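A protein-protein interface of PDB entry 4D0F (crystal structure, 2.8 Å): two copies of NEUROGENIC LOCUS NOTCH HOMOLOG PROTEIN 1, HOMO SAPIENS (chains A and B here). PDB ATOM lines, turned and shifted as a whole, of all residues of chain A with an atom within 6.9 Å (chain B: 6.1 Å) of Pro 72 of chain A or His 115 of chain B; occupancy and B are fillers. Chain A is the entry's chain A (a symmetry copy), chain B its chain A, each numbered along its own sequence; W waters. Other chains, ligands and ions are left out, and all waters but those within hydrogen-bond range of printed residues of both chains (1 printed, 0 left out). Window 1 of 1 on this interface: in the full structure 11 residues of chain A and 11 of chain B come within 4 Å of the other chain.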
ATOM      1  N   CYS A  70       8.140  21.996  13.283  1.00  0.00           N
ATOM      2  CA  CYS A  70       6.732  22.049  13.588  1.00  0.00           C
ATOM      3  C   CYS A  70       5.934  22.909  12.660  1.00  0.00           C
ATOM      4  O   CYS A  70       6.429  23.915  12.142  1.00  0.00           O
ATOM      5  CB  CYS A  70       6.512  22.478  15.037  1.00  0.00           C
ATOM      6  SG  CYS A  70       7.393  21.488  16.267  1.00  0.00           S
ATOM      7  N   MET A  71       4.658  22.528  12.504  1.00  0.00           N
ATOM      8  CA  MET A  71       3.659  23.332  11.830  1.00  0.00           C
ATOM      9  C   MET A  71       3.402  24.517  12.791  1.00  0.00           C
ATOM     10  O   MET A  71       3.558  24.350  14.015  1.00  0.00           O
ATOM     11  CB  MET A  71       2.365  22.527  11.625  1.00  0.00           C
ATOM     12  CG  MET A  71       2.453  21.504  10.529  1.00  0.00           C
ATOM     13  SD  MET A  71       2.184  22.263   8.931  1.00  0.00           S
ATOM     14  CE  MET A  71       3.758  22.215   8.295  1.00  0.00           C
ATOM     15  N   PRO A  72       3.071  25.722  12.267  1.00  0.00           N
ATOM     16  CA  PRO A  72       2.834  26.869  13.165  1.00  0.00           C
ATOM     17  C   PRO A  72       1.842  26.525  14.267  1.00  0.00           C
ATOM     18  O   PRO A  72       0.849  25.851  13.974  1.00  0.00           O
ATOM     19  CB  PRO A  72       2.259  27.947  12.230  1.00  0.00           C
ATOM     20  CG  PRO A  72       1.942  27.264  10.951  1.00  0.00           C
ATOM     21  CD  PRO A  72       2.857  26.092  10.859  1.00  0.00           C
ATOM     22  N   GLY A  73       2.141  26.935  15.500  1.00  0.00           N
ATOM     23  CA  GLY A  73       1.267  26.675  16.640  1.00  0.00           C
ATOM     24  C   GLY A  73       1.602  25.447  17.444  1.00  0.00           C
ATOM     25  O   GLY A  73       0.978  25.190  18.467  1.00  0.00           O
ATOM     26  N   TYR A  74       2.559  24.663  16.970  1.00  0.00           N
ATOM     27  CA  TYR A  74       3.009  23.453  17.658  1.00  0.00           C
ATOM     28  C   TYR A  74       4.460  23.577  18.064  1.00  0.00           C
ATOM     29  O   TYR A  74       5.240  24.296  17.428  1.00  0.00           O
ATOM     30  CB  TYR A  74       2.804  22.209  16.798  1.00  0.00           C
ATOM     31  CG  TYR A  74       1.348  21.937  16.480  1.00  0.00           C
ATOM     32  CD1 TYR A  74       0.525  21.292  17.393  1.00  0.00           C
ATOM     33  CD2 TYR A  74       0.811  22.280  15.242  1.00  0.00           C
ATOM     34  CE1 TYR A  74      -0.810  21.019  17.094  1.00  0.00           C
ATOM     35  CE2 TYR A  74      -0.511  21.986  14.921  1.00  0.00           C
ATOM     36  CZ  TYR A  74      -1.321  21.356  15.851  1.00  0.00           C
ATOM     37  OH  TYR A  74      -2.641  21.059  15.568  1.00  0.00           O
ATOM     38  N   GLU A  75       4.825  22.871  19.132  1.00  0.00           N
ATOM     39  CA  GLU A  75       6.168  22.880  19.683  1.00  0.00           C
ATOM     40  C   GLU A  75       6.490  21.541  20.326  1.00  0.00           C
ATOM     41  O   GLU A  75       5.633  20.659  20.354  1.00  0.00           O
ATOM     42  CB  GLU A  75       6.338  24.062  20.658  1.00  0.00           C
ATOM     43  CG  GLU A  75       5.454  24.041  21.883  1.00  0.00           C
ATOM     44  CD  GLU A  75       5.660  25.253  22.771  1.00  0.00           C
ATOM     45  OE1 GLU A  75       6.793  25.415  23.271  1.00  0.00           O
ATOM     46  OE2 GLU A  75       4.716  26.059  22.946  1.00  0.00           O
ATOM     47  N   THR A  83       0.821  24.839  21.399  1.00  0.00           N
ATOM     48  CA  THR A  83       1.169  26.045  22.176  1.00  0.00           C
ATOM     49  C   THR A  83      -0.094  26.679  22.754  1.00  0.00           C
ATOM     50  O   THR A  83      -1.080  26.836  22.029  1.00  0.00           O
ATOM     51  CB  THR A  83       1.923  27.061  21.298  1.00  0.00           C
ATOM     52  OG1 THR A  83       3.125  26.479  20.768  1.00  0.00           O
ATOM     53  CG2 THR A  83       2.273  28.323  22.061  1.00  0.00           C
ATOM     54  N   GLU A  85      -1.979  29.691  23.415  1.00  0.00           N
ATOM     55  CA  GLU A  85      -2.047  31.122  23.145  1.00  0.00           C
ATOM     56  C   GLU A  85      -2.853  31.914  24.198  1.00  0.00           C
ATOM     57  O   GLU A  85      -2.780  33.151  24.263  1.00  0.00           O
ATOM     58  CB  GLU A  85      -2.536  31.392  21.711  1.00  0.00           C
ATOM     59  CG  GLU A  85      -1.477  31.110  20.637  1.00  0.00           C
ATOM     60  CD  GLU A  85      -1.355  29.677  20.140  1.00  0.00           C
ATOM     61  OE1 GLU A  85      -2.368  28.943  20.203  1.00  0.00           O
ATOM     62  OE2 GLU A  85      -0.264  29.293  19.652  1.00  0.00           O
ATOM     63  N   ILE A 101      -5.247  27.009  16.853  1.00  0.00           N
ATOM     64  CA  ILE A 101      -3.946  26.677  16.305  1.00  0.00           C
ATOM     65  C   ILE A 101      -3.243  27.960  15.894  1.00  0.00           C
ATOM     66  O   ILE A 101      -3.694  28.650  14.983  1.00  0.00           O
ATOM     67  CB  ILE A 101      -4.026  25.605  15.194  1.00  0.00           C
ATOM     68  CG1 ILE A 101      -4.704  24.325  15.735  1.00  0.00           C
ATOM     69  CG2 ILE A 101      -2.635  25.303  14.665  1.00  0.00           C
ATOM     70  CD1 ILE A 101      -5.106  23.334  14.709  1.00  0.00           C
ATOM     71  N   ASN A 102      -2.157  28.292  16.610  1.00  0.00           N
ATOM     72  CA  ASN A 102      -1.333  29.487  16.422  1.00  0.00           C
ATOM     73  C   ASN A 102      -2.156  30.750  16.520  1.00  0.00           C
ATOM     74  O   ASN A 102      -1.848  31.740  15.861  1.00  0.00           O
ATOM     75  CB  ASN A 102      -0.543  29.426  15.109  1.00  0.00           C
ATOM     76  CG  ASN A 102       0.613  30.378  15.052  1.00  0.00           C
ATOM     77  OD1 ASN A 102       1.167  30.758  16.083  1.00  0.00           O
ATOM     78  ND2 ASN A 102       0.966  30.806  13.847  1.00  0.00           N
ATOM     79  N   GLU A 103      -3.210  30.713  17.351  1.00  0.00           N
ATOM     80  CA  GLU A 103      -4.124  31.822  17.576  1.00  0.00           C
ATOM     81  C   GLU A 103      -5.110  31.526  18.696  1.00  0.00           C
ATOM     82  O   GLU A 103      -5.054  30.451  19.286  1.00  0.00           O
ATOM     83  CB  GLU A 103      -4.666  32.440  16.248  1.00  0.00           C
ATOM     84  CG  GLU A 103      -6.158  32.495  15.958  1.00  0.00           C
ATOM     85  CD  GLU A 103      -6.538  31.567  14.826  1.00  0.00           C
ATOM     86  OE1 GLU A 103      -5.947  31.679  13.728  1.00  0.00           O
ATOM     87  OE2 GLU A 103      -7.426  30.714  15.044  1.00  0.00           O
ATOM     88  N   CYS B  91      -0.318  34.264   0.653  1.00  0.00           N
ATOM     89  CA  CYS B  91       0.538  33.106   0.770  1.00  0.00           C
ATOM     90  C   CYS B  91       1.717  33.097  -0.179  1.00  0.00           C
ATOM     91  O   CYS B  91       1.523  33.154  -1.405  1.00  0.00           O
ATOM     92  CB  CYS B  91      -0.271  31.819   0.674  1.00  0.00           C
ATOM     93  SG  CYS B  91      -1.732  31.775   1.753  1.00  0.00           S
ATOM     94  N   GLU B 103      -9.476  36.226   9.537  1.00  0.00           N
ATOM     95  CA  GLU B 103      -8.169  35.616   9.349  1.00  0.00           C
ATOM     96  C   GLU B 103      -8.141  34.696   8.138  1.00  0.00           C
ATOM     97  O   GLU B 103      -9.154  34.555   7.459  1.00  0.00           O
ATOM     98  CB  GLU B 103      -7.537  35.113  10.684  1.00  0.00           C
ATOM     99  CG  GLU B 103      -7.151  33.654  10.871  1.00  0.00           C
ATOM    100  CD  GLU B 103      -8.041  32.968  11.883  1.00  0.00           C
ATOM    101  OE1 GLU B 103      -8.152  33.466  13.027  1.00  0.00           O
ATOM    102  OE2 GLU B 103      -8.641  31.932  11.525  1.00  0.00           O
ATOM    103  N   PHE B 104      -6.957  34.211   7.779  1.00  0.00           N
ATOM    104  CA  PHE B 104      -6.766  33.320   6.647  1.00  0.00           C
ATOM    105  C   PHE B 104      -5.790  32.233   7.043  1.00  0.00           C
ATOM    106  O   PHE B 104      -5.040  32.391   8.015  1.00  0.00           O
ATOM    107  CB  PHE B 104      -6.242  34.075   5.408  1.00  0.00           C
ATOM    108  CG  PHE B 104      -4.882  34.696   5.596  1.00  0.00           C
ATOM    109  CD1 PHE B 104      -3.719  33.959   5.360  1.00  0.00           C
ATOM    110  CD2 PHE B 104      -4.759  36.004   6.047  1.00  0.00           C
ATOM    111  CE1 PHE B 104      -2.473  34.527   5.549  1.00  0.00           C
ATOM    112  CE2 PHE B 104      -3.508  36.572   6.233  1.00  0.00           C
ATOM    113  CZ  PHE B 104      -2.379  35.836   5.971  1.00  0.00           C
ATOM    114  N   GLN B 105      -5.777  31.152   6.258  1.00  0.00           N
ATOM    115  CA  GLN B 105      -4.908  30.024   6.451  1.00  0.00           C
ATOM    116  C   GLN B 105      -4.238  29.774   5.121  1.00  0.00           C
ATOM    117  O   GLN B 105      -4.894  29.793   4.072  1.00  0.00           O
ATOM    118  CB  GLN B 105      -5.740  28.801   6.889  1.00  0.00           C
ATOM    119  CG  GLN B 105      -4.951  27.575   7.342  1.00  0.00           C
ATOM    120  CD  GLN B 105      -5.785  26.306   7.276  1.00  0.00           C
ATOM    121  OE1 GLN B 105      -6.982  26.292   7.627  1.00  0.00           O
ATOM    122  NE2 GLN B 105      -5.166  25.197   6.840  1.00  0.00           N
ATOM    123  N   CYS B 106      -2.920  29.530   5.175  1.00  0.00           N
ATOM    124  CA  CYS B 106      -2.153  29.161   4.007  1.00  0.00           C
ATOM    125  C   CYS B 106      -1.904  27.664   4.016  1.00  0.00           C
ATOM    126  O   CYS B 106      -1.422  27.108   5.005  1.00  0.00           O
ATOM    127  CB  CYS B 106      -0.850  29.941   3.926  1.00  0.00           C
ATOM    128  SG  CYS B 106      -1.070  31.712   3.665  1.00  0.00           S
ATOM    129  N   CYS B 108       0.432  25.360   2.553  1.00  0.00           N
ATOM    130  CA  CYS B 108       1.753  25.385   1.946  1.00  0.00           C
ATOM    131  C   CYS B 108       2.034  24.138   1.151  1.00  0.00           C
ATOM    132  O   CYS B 108       1.646  23.053   1.584  1.00  0.00           O
ATOM    133  CB  CYS B 108       2.829  25.607   3.009  1.00  0.00           C
ATOM    134  SG  CYS B 108       2.631  27.110   3.990  1.00  0.00           S
ATOM    135  N   THR B 113       6.695  25.998   5.185  1.00  0.00           N
ATOM    136  CA  THR B 113       5.909  26.258   6.444  1.00  0.00           C
ATOM    137  C   THR B 113       6.195  27.784   6.718  1.00  0.00           C
ATOM    138  O   THR B 113       7.113  28.266   6.092  1.00  0.00           O
ATOM    139  CB  THR B 113       6.424  25.311   7.532  1.00  0.00           C
ATOM    140  OG1 THR B 113       6.335  23.983   7.045  1.00  0.00           O
ATOM    141  CG2 THR B 113       5.661  25.401   8.810  1.00  0.00           C
ATOM    142  N   GLY B 114       5.463  28.619   7.450  1.00  0.00           N
ATOM    143  CA  GLY B 114       4.312  28.503   8.316  1.00  0.00           C
ATOM    144  C   GLY B 114       3.194  29.412   7.873  1.00  0.00           C
ATOM    145  O   GLY B 114       2.672  29.180   6.793  1.00  0.00           O
ATOM    146  N   HIS B 115       2.790  30.403   8.693  1.00  0.00           N
ATOM    147  CA  HIS B 115       1.633  31.246   8.419  1.00  0.00           C
ATOM    148  C   HIS B 115       1.451  31.736   7.008  1.00  0.00           C
ATOM    149  O   HIS B 115       0.343  31.655   6.464  1.00  0.00           O
ATOM    150  CB  HIS B 115       1.461  32.385   9.408  1.00  0.00           C
ATOM    151  CG  HIS B 115       0.056  32.905   9.384  1.00  0.00           C
ATOM    152  ND1 HIS B 115      -0.255  34.127   8.830  1.00  0.00           N
ATOM    153  CD2 HIS B 115      -1.090  32.286   9.745  1.00  0.00           C
ATOM    154  CE1 HIS B 115      -1.562  34.248   8.953  1.00  0.00           C
ATOM    155  NE2 HIS B 115      -2.108  33.162   9.487  1.00  0.00           N
ATOM    156  N   LEU B 116       2.526  32.254   6.430  1.00  0.00           N
ATOM    157  CA  LEU B 116       2.513  32.780   5.082  1.00  0.00           C
ATOM    158  C   LEU B 116       3.397  31.936   4.167  1.00  0.00           C
ATOM    159  O   LEU B 116       3.730  32.391   3.065  1.00  0.00           O
ATOM    160  CB  LEU B 116       2.970  34.244   5.099  1.00  0.00           C
ATOM    161  CG  LEU B 116       2.110  35.218   5.883  1.00  0.00           C
ATOM    162  CD1 LEU B 116       2.904  36.420   6.319  1.00  0.00           C
ATOM    163  CD2 LEU B 116       0.985  35.699   5.088  1.00  0.00           C
ATOM    164  N   CYS B 117       3.782  30.704   4.615  1.00  0.00           N
ATOM    165  CA  CYS B 117       4.654  29.768   3.881  1.00  0.00           C
ATOM    166  C   CYS B 117       6.044  30.364   3.700  1.00  0.00           C
ATOM    167  O   CYS B 117       6.683  30.086   2.692  1.00  0.00           O
ATOM    168  CB  CYS B 117       4.043  29.374   2.536  1.00  0.00           C
ATOM    169  SG  CYS B 117       2.403  28.636   2.653  1.00  0.00           S
ATOM    170  N   GLN B 118       6.513  31.193   4.652  1.00  0.00           N
ATOM    171  CA  GLN B 118       7.816  31.861   4.540  1.00  0.00           C
ATOM    172  C   GLN B 118       8.994  30.888   4.569  1.00  0.00           C
ATOM    173  O   GLN B 118       9.950  31.071   3.821  1.00  0.00           O
ATOM    174  CB  GLN B 118       8.078  32.837   5.697  1.00  0.00           C
ATOM    175  CG  GLN B 118       7.079  33.891   6.006  1.00  0.00           C
ATOM    176  CD  GLN B 118       6.043  33.406   7.001  1.00  0.00           C
ATOM    177  OE1 GLN B 118       5.849  32.201   7.235  1.00  0.00           O
ATOM    178  NE2 GLN B 118       5.301  34.352   7.570  1.00  0.00           N
HETATM  179  O   HOH W   1      -4.589  31.314  10.551  1.00  0.00           O
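Glu 103 of chain A touches its own counterpart, Glu 103 of chain B.
Of the 6 pairs that touch across the chains among the printed residues, 1 has its exchanged pair printed and touching as well.
The backbone carbonyl oxygen (O) of Phe 104 of chain B lies within hydrogen-bond range of a ring nitrogen (NE2) of His 115 of chain B, 3.4 Å away.
The backbone NH (N) of Gln 118 of chain B lies within hydrogen-bond range of the backbone carbonyl oxygen (O) of Thr 113 of chain B, at 3.3 Å.
OE1 of Glu 85 of chain A lies close to N of Glu 103 of chain A (3.5 Å).
SG of Cys 91 of chain B is disulfide-bonded to SG of Cys 106 of chain B (2.0 Å).
The side-chain sulfur (SG) of Cys 117 of chain B forms a disulfide with the side-chain sulfur (SG) of Cys 108 of chain B (2.0 Å).
Of the 11 printed residues of chain A, 4 touch a printed residue of chain B.
Hydrophobic or aromatic side chains of chain A within 4 Å of the printed part of chain B: Met 71 and Pro 72.
Water W1 lies within hydrogen-bond range of the backbone carbonyl oxygen of Phe 104 of chain B (2.8 Å), a ring nitrogen (NE2) of His 115 of chain B (3.3 Å) and the side-chain carboxylate of Glu 103 of chain A (3.5 Å).
Of chain A, only Pro 72 (3.96 Å) comes within 4 Å of His 115 of chain B.
Of the printed residues of chain A, Gly 114 of chain B touches Pro 72 (3.8 Å).
Of the printed residues of chain B, Cys 70 of chain A touches Thr 113.
Of the printed residues of chain B, Met 71 of chain A touches Thr 113.
Of the printed residues of chain B, Glu 103 of chain A touches Glu 103 (2.9 Å).
Of the printed residues of chain A, Thr 113 of chain B touches Cys 70 (3.7 Å), Met 71 (3.4 Å) and Pro 72 (3.5 Å).
The nearest printed residue of chain B that does not touch Pro 72 of chain A is Leu 116 of chain B (6.8 Å).
O of Cys 70 of chain A touches CG2 of Thr 113 of chain B, 3.7 Å away.
Met 71 of chain A touches Thr 113 of chain B (CE to OG1, 3.4 Å).
Pro 72 of chain A touches Thr 113 of chain B.
Pro 72 of chain A touches Gly 114 of chain B.
Pro 72 of chain A touches His 115 of chain B.
The side-chain carboxylate of Glu 103 of chain B lies close to the side-chain carboxylate of Glu 103 of chain A, 2.9 Å away.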
